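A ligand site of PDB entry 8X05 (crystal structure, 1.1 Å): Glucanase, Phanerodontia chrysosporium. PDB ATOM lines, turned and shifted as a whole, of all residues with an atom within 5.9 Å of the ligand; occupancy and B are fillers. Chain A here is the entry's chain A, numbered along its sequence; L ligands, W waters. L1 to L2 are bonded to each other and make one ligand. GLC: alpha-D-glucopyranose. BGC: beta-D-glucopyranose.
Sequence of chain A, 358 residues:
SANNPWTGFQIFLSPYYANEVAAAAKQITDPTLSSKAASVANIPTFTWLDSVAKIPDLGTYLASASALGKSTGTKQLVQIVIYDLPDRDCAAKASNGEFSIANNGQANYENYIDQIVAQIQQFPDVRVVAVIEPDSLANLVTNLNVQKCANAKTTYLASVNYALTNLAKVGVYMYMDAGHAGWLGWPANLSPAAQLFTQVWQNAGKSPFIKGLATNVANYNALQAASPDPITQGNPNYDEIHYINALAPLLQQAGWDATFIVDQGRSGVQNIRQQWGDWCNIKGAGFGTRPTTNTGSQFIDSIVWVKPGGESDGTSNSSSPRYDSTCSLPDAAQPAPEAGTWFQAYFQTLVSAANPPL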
ATOM      1  N   TYR A  83      -7.005   5.024 -19.944  1.00  0.00           N
ATOM      2  CA  TYR A  83      -6.783   3.598 -20.205  1.00  0.00           C
ATOM      3  C   TYR A  83      -5.744   3.043 -19.223  1.00  0.00           C
ATOM      4  O   TYR A  83      -4.618   2.702 -19.592  1.00  0.00           O
ATOM      5  CB  TYR A  83      -6.367   3.356 -21.653  1.00  0.00           C
ATOM      6  CG  TYR A  83      -6.303   1.891 -22.034  1.00  0.00           C
ATOM      7  CD1 TYR A  83      -7.437   1.079 -21.929  1.00  0.00           C
ATOM      8  CD2 TYR A  83      -5.120   1.317 -22.494  1.00  0.00           C
ATOM      9  CE1 TYR A  83      -7.393  -0.265 -22.280  1.00  0.00           C
ATOM     10  CE2 TYR A  83      -5.070  -0.015 -22.850  1.00  0.00           C
ATOM     11  CZ  TYR A  83      -6.196  -0.804 -22.744  1.00  0.00           C
ATOM     12  OH  TYR A  83      -6.129  -2.133 -23.109  1.00  0.00           O
ATOM     13  N   ASP A  89      -7.857  -5.030 -19.294  1.00  0.00           N
ATOM     14  CA  ASP A  89      -7.963  -6.011 -20.382  1.00  0.00           C
ATOM     15  C   ASP A  89      -8.261  -7.401 -19.826  1.00  0.00           C
ATOM     16  O   ASP A  89      -7.521  -8.354 -20.051  1.00  0.00           O
ATOM     17  CB  ASP A  89      -6.676  -6.022 -21.213  1.00  0.00           C
ATOM     18  CG  ASP A  89      -6.845  -6.541 -22.638  1.00  0.00           C
ATOM     19  OD1 ASP A  89      -7.982  -6.663 -23.150  1.00  0.00           O
ATOM     20  OD2 ASP A  89      -5.793  -6.820 -23.255  1.00  0.00           O
ATOM     21  N   ALA A  91     -10.296  -9.868 -20.355  1.00  0.00           N
ATOM     22  CA  ALA A  91     -10.626 -11.046 -21.160  1.00  0.00           C
ATOM     23  C   ALA A  91      -9.555 -11.367 -22.195  1.00  0.00           C
ATOM     24  O   ALA A  91      -9.793 -12.178 -23.097  1.00  0.00           O
ATOM     25  CB  ALA A  91     -11.988 -10.867 -21.852  1.00  0.00           C
ATOM     26  N   ALA A  92      -8.389 -10.747 -22.094  1.00  0.00           N
ATOM     27  CA  ALA A  92      -7.277 -10.984 -22.997  1.00  0.00           C
ATOM     28  C   ALA A  92      -6.000 -10.782 -22.207  1.00  0.00           C
ATOM     29  O   ALA A  92      -6.030 -10.416 -21.027  1.00  0.00           O
ATOM     30  CB  ALA A  92      -7.342 -10.075 -24.238  1.00  0.00           C
ATOM     31  N   ASP A 135     -12.798  -1.304 -23.723  1.00  0.00           N
ATOM     32  CA  ASP A 135     -13.060  -2.722 -23.460  1.00  0.00           C
ATOM     33  C   ASP A 135     -13.692  -3.008 -22.103  1.00  0.00           C
ATOM     34  O   ASP A 135     -14.310  -4.057 -21.938  1.00  0.00           O
ATOM     35  CB  ASP A 135     -11.790  -3.574 -23.577  1.00  0.00           C
ATOM     36  CG  ASP A 135     -11.162  -3.517 -24.940  1.00  0.00           C
ATOM     37  OD1 ASP A 135     -11.865  -3.221 -25.928  1.00  0.00           O
ATOM     38  OD2 ASP A 135      -9.942  -3.737 -25.018  1.00  0.00           O
ATOM     39  N   ASN A 139     -16.660  -5.759 -21.459  1.00  0.00           N
ATOM     40  CA  ASN A 139     -16.369  -7.012 -20.774  1.00  0.00           C
ATOM     41  C   ASN A 139     -17.349  -7.280 -19.638  1.00  0.00           C
ATOM     42  O   ASN A 139     -17.665  -8.441 -19.357  1.00  0.00           O
ATOM     43  CB  ASN A 139     -14.934  -7.011 -20.245  1.00  0.00           C
ATOM     44  CG  ASN A 139     -13.922  -7.410 -21.292  1.00  0.00           C
ATOM     45  OD1 ASN A 139     -14.145  -8.331 -22.076  1.00  0.00           O
ATOM     46  ND2 ASN A 139     -12.794  -6.716 -21.300  1.00  0.00           N
ATOM     47  N   THR A 142     -20.713  -8.810 -21.383  1.00  0.00           N
ATOM     48  CA  THR A 142     -20.742 -10.151 -21.959  1.00  0.00           C
ATOM     49  C   THR A 142     -19.795 -11.152 -21.326  1.00  0.00           C
ATOM     50  O   THR A 142     -19.970 -12.354 -21.556  1.00  0.00           O
ATOM     51  CB  THR A 142     -20.448 -10.128 -23.471  1.00  0.00           C
ATOM     52  OG1 THR A 142     -19.049  -9.892 -23.685  1.00  0.00           O
ATOM     53  CG2 THR A 142     -21.242  -9.045 -24.195  1.00  0.00           C
ATOM     54  N   ASN A 143     -18.822 -10.725 -20.527  1.00  0.00           N
ATOM     55  CA  ASN A 143     -17.764 -11.647 -20.133  1.00  0.00           C
ATOM     56  C   ASN A 143     -17.638 -11.824 -18.622  1.00  0.00           C
ATOM     57  O   ASN A 143     -16.546 -12.056 -18.116  1.00  0.00           O
ATOM     58  CB  ASN A 143     -16.448 -11.265 -20.800  1.00  0.00           C
ATOM     59  CG  ASN A 143     -16.594 -11.174 -22.295  1.00  0.00           C
ATOM     60  OD1 ASN A 143     -17.465 -11.836 -22.879  1.00  0.00           O
ATOM     61  ND2 ASN A 143     -15.784 -10.345 -22.924  1.00  0.00           N
ATOM     62  N   HIS A 180     -18.045  -2.763 -30.007  1.00  0.00           N
ATOM     63  CA  HIS A 180     -18.324  -2.564 -31.427  1.00  0.00           C
ATOM     64  C   HIS A 180     -19.489  -3.457 -31.810  1.00  0.00           C
ATOM     65  O   HIS A 180     -20.027  -4.201 -30.979  1.00  0.00           O
ATOM     66  CB  HIS A 180     -17.081  -2.806 -32.279  1.00  0.00           C
ATOM     67  CG  HIS A 180     -16.529  -4.188 -32.155  1.00  0.00           C
ATOM     68  ND1 HIS A 180     -16.991  -5.240 -32.922  1.00  0.00           N
ATOM     69  CD2 HIS A 180     -15.570  -4.706 -31.356  1.00  0.00           C
ATOM     70  CE1 HIS A 180     -16.336  -6.341 -32.601  1.00  0.00           C
ATOM     71  NE2 HIS A 180     -15.473  -6.042 -31.645  1.00  0.00           N
ATOM     72  N   GLY A 182     -19.763  -6.185 -33.459  1.00  0.00           N
ATOM     73  CA  GLY A 182     -19.560  -7.605 -33.250  1.00  0.00           C
ATOM     74  C   GLY A 182     -19.436  -8.016 -31.813  1.00  0.00           C
ATOM     75  O   GLY A 182     -19.322  -9.225 -31.537  1.00  0.00           O
ATOM     76  N   TRP A 183     -19.455  -7.060 -30.885  1.00  0.00           N
ATOM     77  CA  TRP A 183     -19.366  -7.315 -29.453  1.00  0.00           C
ATOM     78  C   TRP A 183     -20.698  -7.039 -28.780  1.00  0.00           C
ATOM     79  O   TRP A 183     -21.388  -7.970 -28.356  1.00  0.00           O
ATOM     80  CB  TRP A 183     -18.238  -6.463 -28.851  1.00  0.00           C
ATOM     81  CG  TRP A 183     -17.818  -6.899 -27.472  1.00  0.00           C
ATOM     82  CD1 TRP A 183     -18.487  -7.746 -26.625  1.00  0.00           C
ATOM     83  CD2 TRP A 183     -16.637  -6.501 -26.768  1.00  0.00           C
ATOM     84  NE1 TRP A 183     -17.794  -7.904 -25.447  1.00  0.00           N
ATOM     85  CE2 TRP A 183     -16.648  -7.158 -25.509  1.00  0.00           C
ATOM     86  CE3 TRP A 183     -15.561  -5.650 -27.078  1.00  0.00           C
ATOM     87  CZ2 TRP A 183     -15.626  -6.996 -24.566  1.00  0.00           C
ATOM     88  CZ3 TRP A 183     -14.541  -5.500 -26.143  1.00  0.00           C
ATOM     89  CH2 TRP A 183     -14.591  -6.168 -24.897  1.00  0.00           C
ATOM     90  N   VAL A 217     -13.392   1.160 -31.163  1.00  0.00           N
ATOM     91  CA  VAL A 217     -12.047   1.572 -30.754  1.00  0.00           C
ATOM     92  C   VAL A 217     -11.093   0.393 -30.878  1.00  0.00           C
ATOM     93  O   VAL A 217     -11.341  -0.699 -30.351  1.00  0.00           O
ATOM     94  CB  VAL A 217     -12.049   2.093 -29.304  1.00  0.00           C
ATOM     95  CG1 VAL A 217     -10.624   2.356 -28.825  1.00  0.00           C
ATOM     96  CG2 VAL A 217     -12.913   3.338 -29.159  1.00  0.00           C
ATOM     97  N   ALA A 218      -9.993   0.625 -31.579  1.00  0.00           N
ATOM     98  CA  ALA A 218      -8.995  -0.401 -31.845  1.00  0.00           C
ATOM     99  C   ALA A 218      -9.539  -1.571 -32.661  1.00  0.00           C
ATOM    100  O   ALA A 218      -8.924  -2.642 -32.711  1.00  0.00           O
ATOM    101  CB  ALA A 218      -8.263  -0.894 -30.593  1.00  0.00           C
ATOM    102  N   ASN A 219     -10.683  -1.396 -33.310  1.00  0.00           N
ATOM    103  CA  ASN A 219     -11.226  -2.444 -34.163  1.00  0.00           C
ATOM    104  C   ASN A 219     -11.222  -1.972 -35.618  1.00  0.00           C
ATOM    105  O   ASN A 219     -10.582  -0.965 -35.977  1.00  0.00           O
ATOM    106  CB  ASN A 219     -12.568  -2.949 -33.639  1.00  0.00           C
ATOM    107  CG  ASN A 219     -12.797  -4.423 -33.990  1.00  0.00           C
ATOM    108  OD1 ASN A 219     -13.141  -4.744 -35.124  1.00  0.00           O
ATOM    109  ND2 ASN A 219     -12.568  -5.315 -33.022  1.00  0.00           N
ATOM    110  N   ARG A 273     -10.409 -10.336 -42.092  1.00  0.00           N
ATOM    111  CA  ARG A 273     -10.568 -11.161 -40.918  1.00  0.00           C
ATOM    112  C   ARG A 273     -11.254 -12.481 -41.273  1.00  0.00           C
ATOM    113  O   ARG A 273     -12.272 -12.497 -41.977  1.00  0.00           O
ATOM    114  CB  ARG A 273     -11.387 -10.443 -39.838  1.00  0.00           C
ATOM    115  CG  ARG A 273     -10.597  -9.395 -39.104  1.00  0.00           C
ATOM    116  CD  ARG A 273     -11.469  -8.654 -38.094  1.00  0.00           C
ATOM    117  NE  ARG A 273     -12.423  -7.757 -38.714  1.00  0.00           N
ATOM    118  CZ  ARG A 273     -13.201  -6.929 -38.038  1.00  0.00           C
ATOM    119  NH1 ARG A 273     -13.181  -6.890 -36.713  1.00  0.00           N
ATOM    120  NH2 ARG A 273     -14.012  -6.104 -38.700  1.00  0.00           N
ATOM    121  N   TRP A 276     -14.885 -12.695 -36.854  1.00  0.00           N
ATOM    122  CA  TRP A 276     -15.143 -11.349 -36.343  1.00  0.00           C
ATOM    123  C   TRP A 276     -14.306 -11.042 -35.105  1.00  0.00           C
ATOM    124  O   TRP A 276     -13.848  -9.909 -34.929  1.00  0.00           O
ATOM    125  CB  TRP A 276     -16.608 -11.167 -36.004  1.00  0.00           C
ATOM    126  CG  TRP A 276     -17.082  -9.750 -36.185  1.00  0.00           C
ATOM    127  CD1 TRP A 276     -16.313  -8.620 -36.337  1.00  0.00           C
ATOM    128  CD2 TRP A 276     -18.441  -9.329 -36.251  1.00  0.00           C
ATOM    129  NE1 TRP A 276     -17.127  -7.522 -36.480  1.00  0.00           N
ATOM    130  CE2 TRP A 276     -18.432  -7.926 -36.435  1.00  0.00           C
ATOM    131  CE3 TRP A 276     -19.668  -9.988 -36.157  1.00  0.00           C
ATOM    132  CZ2 TRP A 276     -19.603  -7.183 -36.545  1.00  0.00           C
ATOM    133  CZ3 TRP A 276     -20.817  -9.259 -36.253  1.00  0.00           C
ATOM    134  CH2 TRP A 276     -20.786  -7.872 -36.443  1.00  0.00           C
ATOM    135  N   GLY A 277     -14.114 -12.035 -34.246  1.00  0.00           N
ATOM    136  CA  GLY A 277     -13.374 -11.857 -33.024  1.00  0.00           C
ATOM    137  C   GLY A 277     -11.870 -11.795 -33.173  1.00  0.00           C
ATOM    138  O   GLY A 277     -11.154 -11.736 -32.175  1.00  0.00           O
ATOM    139  N   ASP A 278     -11.353 -11.806 -34.401  1.00  0.00           N
ATOM    140  CA  ASP A 278      -9.914 -11.653 -34.617  1.00  0.00           C
ATOM    141  C   ASP A 278      -9.605 -10.163 -34.544  1.00  0.00           C
ATOM    142  O   ASP A 278      -9.843  -9.417 -35.499  1.00  0.00           O
ATOM    143  CB  ASP A 278      -9.516 -12.192 -35.994  1.00  0.00           C
ATOM    144  CG  ASP A 278      -9.828 -13.670 -36.157  1.00  0.00           C
ATOM    145  OD1 ASP A 278     -10.116 -14.357 -35.154  1.00  0.00           O
ATOM    146  OD2 ASP A 278      -9.773 -14.152 -37.314  1.00  0.00           O
ATOM    147  N   TRP A 279      -9.079  -9.703 -33.403  1.00  0.00           N
ATOM    148  CA  TRP A 279      -8.890  -8.278 -33.146  1.00  0.00           C
ATOM    149  C   TRP A 279      -7.452  -7.804 -33.237  1.00  0.00           C
ATOM    150  O   TRP A 279      -7.217  -6.594 -33.195  1.00  0.00           O
ATOM    151  CB  TRP A 279      -9.436  -7.888 -31.758  1.00  0.00           C
ATOM    152  CG  TRP A 279      -8.953  -8.777 -30.653  1.00  0.00           C
ATOM    153  CD1 TRP A 279      -9.624  -9.838 -30.110  1.00  0.00           C
ATOM    154  CD2 TRP A 279      -7.705  -8.704 -29.948  1.00  0.00           C
ATOM    155  NE1 TRP A 279      -8.874 -10.433 -29.128  1.00  0.00           N
ATOM    156  CE2 TRP A 279      -7.691  -9.756 -29.013  1.00  0.00           C
ATOM    157  CE3 TRP A 279      -6.590  -7.854 -30.028  1.00  0.00           C
ATOM    158  CZ2 TRP A 279      -6.611  -9.980 -28.153  1.00  0.00           C
ATOM    159  CZ3 TRP A 279      -5.530  -8.074 -29.183  1.00  0.00           C
ATOM    160  CH2 TRP A 279      -5.550  -9.135 -28.252  1.00  0.00           C
HETATM  161  C1  GLC L   1     -15.776 -10.543 -29.761  1.00  0.00           C
HETATM  162  C2  GLC L   1     -15.245  -9.217 -30.292  1.00  0.00           C
HETATM  163  C3  GLC L   1     -13.887  -8.928 -29.797  1.00  0.00           C
HETATM  164  C4  GLC L   1     -13.813  -8.984 -28.297  1.00  0.00           C
HETATM  165  C5  GLC L   1     -14.448 -10.261 -27.727  1.00  0.00           C
HETATM  166  C6  GLC L   1     -14.548 -10.102 -26.233  1.00  0.00           C
HETATM  167  O1  GLC L   1     -14.972 -11.539 -30.189  1.00  0.00           O
HETATM  168  O2  GLC L   1     -15.195  -9.248 -31.721  1.00  0.00           O
HETATM  169  O3  GLC L   1     -13.544  -7.604 -30.294  1.00  0.00           O
HETATM  170  O4  GLC L   1     -12.455  -9.053 -27.875  1.00  0.00           O
HETATM  171  O5  GLC L   1     -15.784 -10.548 -28.266  1.00  0.00           O
HETATM  172  O6  GLC L   1     -14.321 -11.321 -25.569  1.00  0.00           O
HETATM  173  C2  BGC L   2     -10.617  -8.045 -26.687  1.00  0.00           C
HETATM  174  C3  BGC L   2      -9.881  -6.783 -26.412  1.00  0.00           C
HETATM  175  C4  BGC L   2      -9.711  -5.928 -27.642  1.00  0.00           C
HETATM  176  C5  BGC L   2     -11.068  -5.675 -28.318  1.00  0.00           C
HETATM  177  C6  BGC L   2     -10.922  -4.914 -29.608  1.00  0.00           C
HETATM  178  C1  BGC L   2     -11.896  -7.812 -27.464  1.00  0.00           C
HETATM  179  O2  BGC L   2     -10.942  -8.720 -25.443  1.00  0.00           O
HETATM  180  O3  BGC L   2      -8.583  -7.103 -25.851  1.00  0.00           O
HETATM  181  O4  BGC L   2      -9.060  -4.693 -27.320  1.00  0.00           O
HETATM  182  O5  BGC L   2     -11.652  -6.977 -28.647  1.00  0.00           O
HETATM  183  O6  BGC L   2     -12.177  -4.733 -30.227  1.00  0.00           O
HETATM  184  O   HOH W   1     -12.850  -8.196 -33.101  1.00  0.00           O
HETATM  185  O   HOH W   2      -6.903  -4.129 -28.655  1.00  0.00           O
HETATM  186  O   HOH W   3     -10.395  -7.950 -22.716  1.00  0.00           O
HETATM  187  O   HOH W   4     -11.254 -11.417 -25.465  1.00  0.00           O
HETATM  188  O   HOH W   5     -17.383 -10.526 -32.763  1.00  0.00           O
HETATM  189  O   HOH W   6     -11.948 -12.733 -29.870  1.00  0.00           O
HETATM  190  O   HOH W   7     -13.470  -2.414 -29.716  1.00  0.00           O
HETATM  191  O   HOH W   8      -5.909  -7.217 -25.781  1.00  0.00           O
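The side-chain amide oxygen (OD1) of Asn 143 lies within hydrogen-bond range of the side-chain hydroxyl (OG1) of Thr 142, at 2.6 Å.
NE1 of Trp 183 sits at hydrogen-bond distance from OG1 of Thr 142 (2.9 Å).
NE2 of His 180 lies within hydrogen-bond range of ND2 of Asn 219 (3.3 Å).
The backbone NH (N) of Gly 182 sits at hydrogen-bond distance from a ring nitrogen (ND1) of His 180 (3.0 Å).
OD1 of Asn 219 lies within hydrogen-bond range of NH1 of Arg 273 (2.7 Å).
The side-chain amide nitrogen of Asn 143 sits at hydrogen-bond distance from the side-chain amide oxygen of Asn 139, at 2.7 Å.
O of Asp 135 is in hydrogen-bond range of ND2 of Asn 139, at 3.1 Å.
Residues that only touch the ligand: Gly 277, Trp 276, Ala 92, Trp 183 and Trp 279.
Hydrophobic or aromatic side chains within 4 Å of the ligand: Ala 92, His 180, Trp 183 and Trp 279.
The nearest printed residue that does not touch the ligand is Val 217 (4.1 Å).
Water W8 bridges OD2 of Asp 89 and O3 of BGC L2.
Water W7 bridges O6 of BGC L2 (2.7 Å) and O of Val 217 (2.8 Å).
Water W4 bridges an oxygen (O2) of BGC L2 (2.7 Å) and the backbone carbonyl oxygen of Ala 91 (2.9 Å).
Water W5 bridges the backbone carbonyl oxygen of Gly 182 (2.6 Å) and an oxygen (O2) of GLC L1 (2.7 Å).
Water W1 lies within hydrogen-bond range of O of Trp 276, ND2 of Asn 219 and O2 of GLC L1.
Water W6 bridges O of Gly 277 (2.6 Å) and O1 of GLC L1 (3.3 Å).
The side-chain amide nitrogen (ND2) of Asn 219 lies within hydrogen-bond range of an oxygen (O6) of BGC L2.
OD1 of Asp 89 lies within hydrogen-bond range of O3 of BGC L2, 2.8 Å away.
The side-chain carboxylate (OD2) of Asp 135 lies within hydrogen-bond range of an oxygen (O4) of BGC L2 (2.6 Å).
NE2 of His 180 sits at hydrogen-bond distance from O3 of GLC L1 (2.8 Å).
The side-chain amide nitrogen (ND2) of Asn 143 sits at hydrogen-bond distance from an oxygen (O6) of GLC L1 (3.2 Å).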
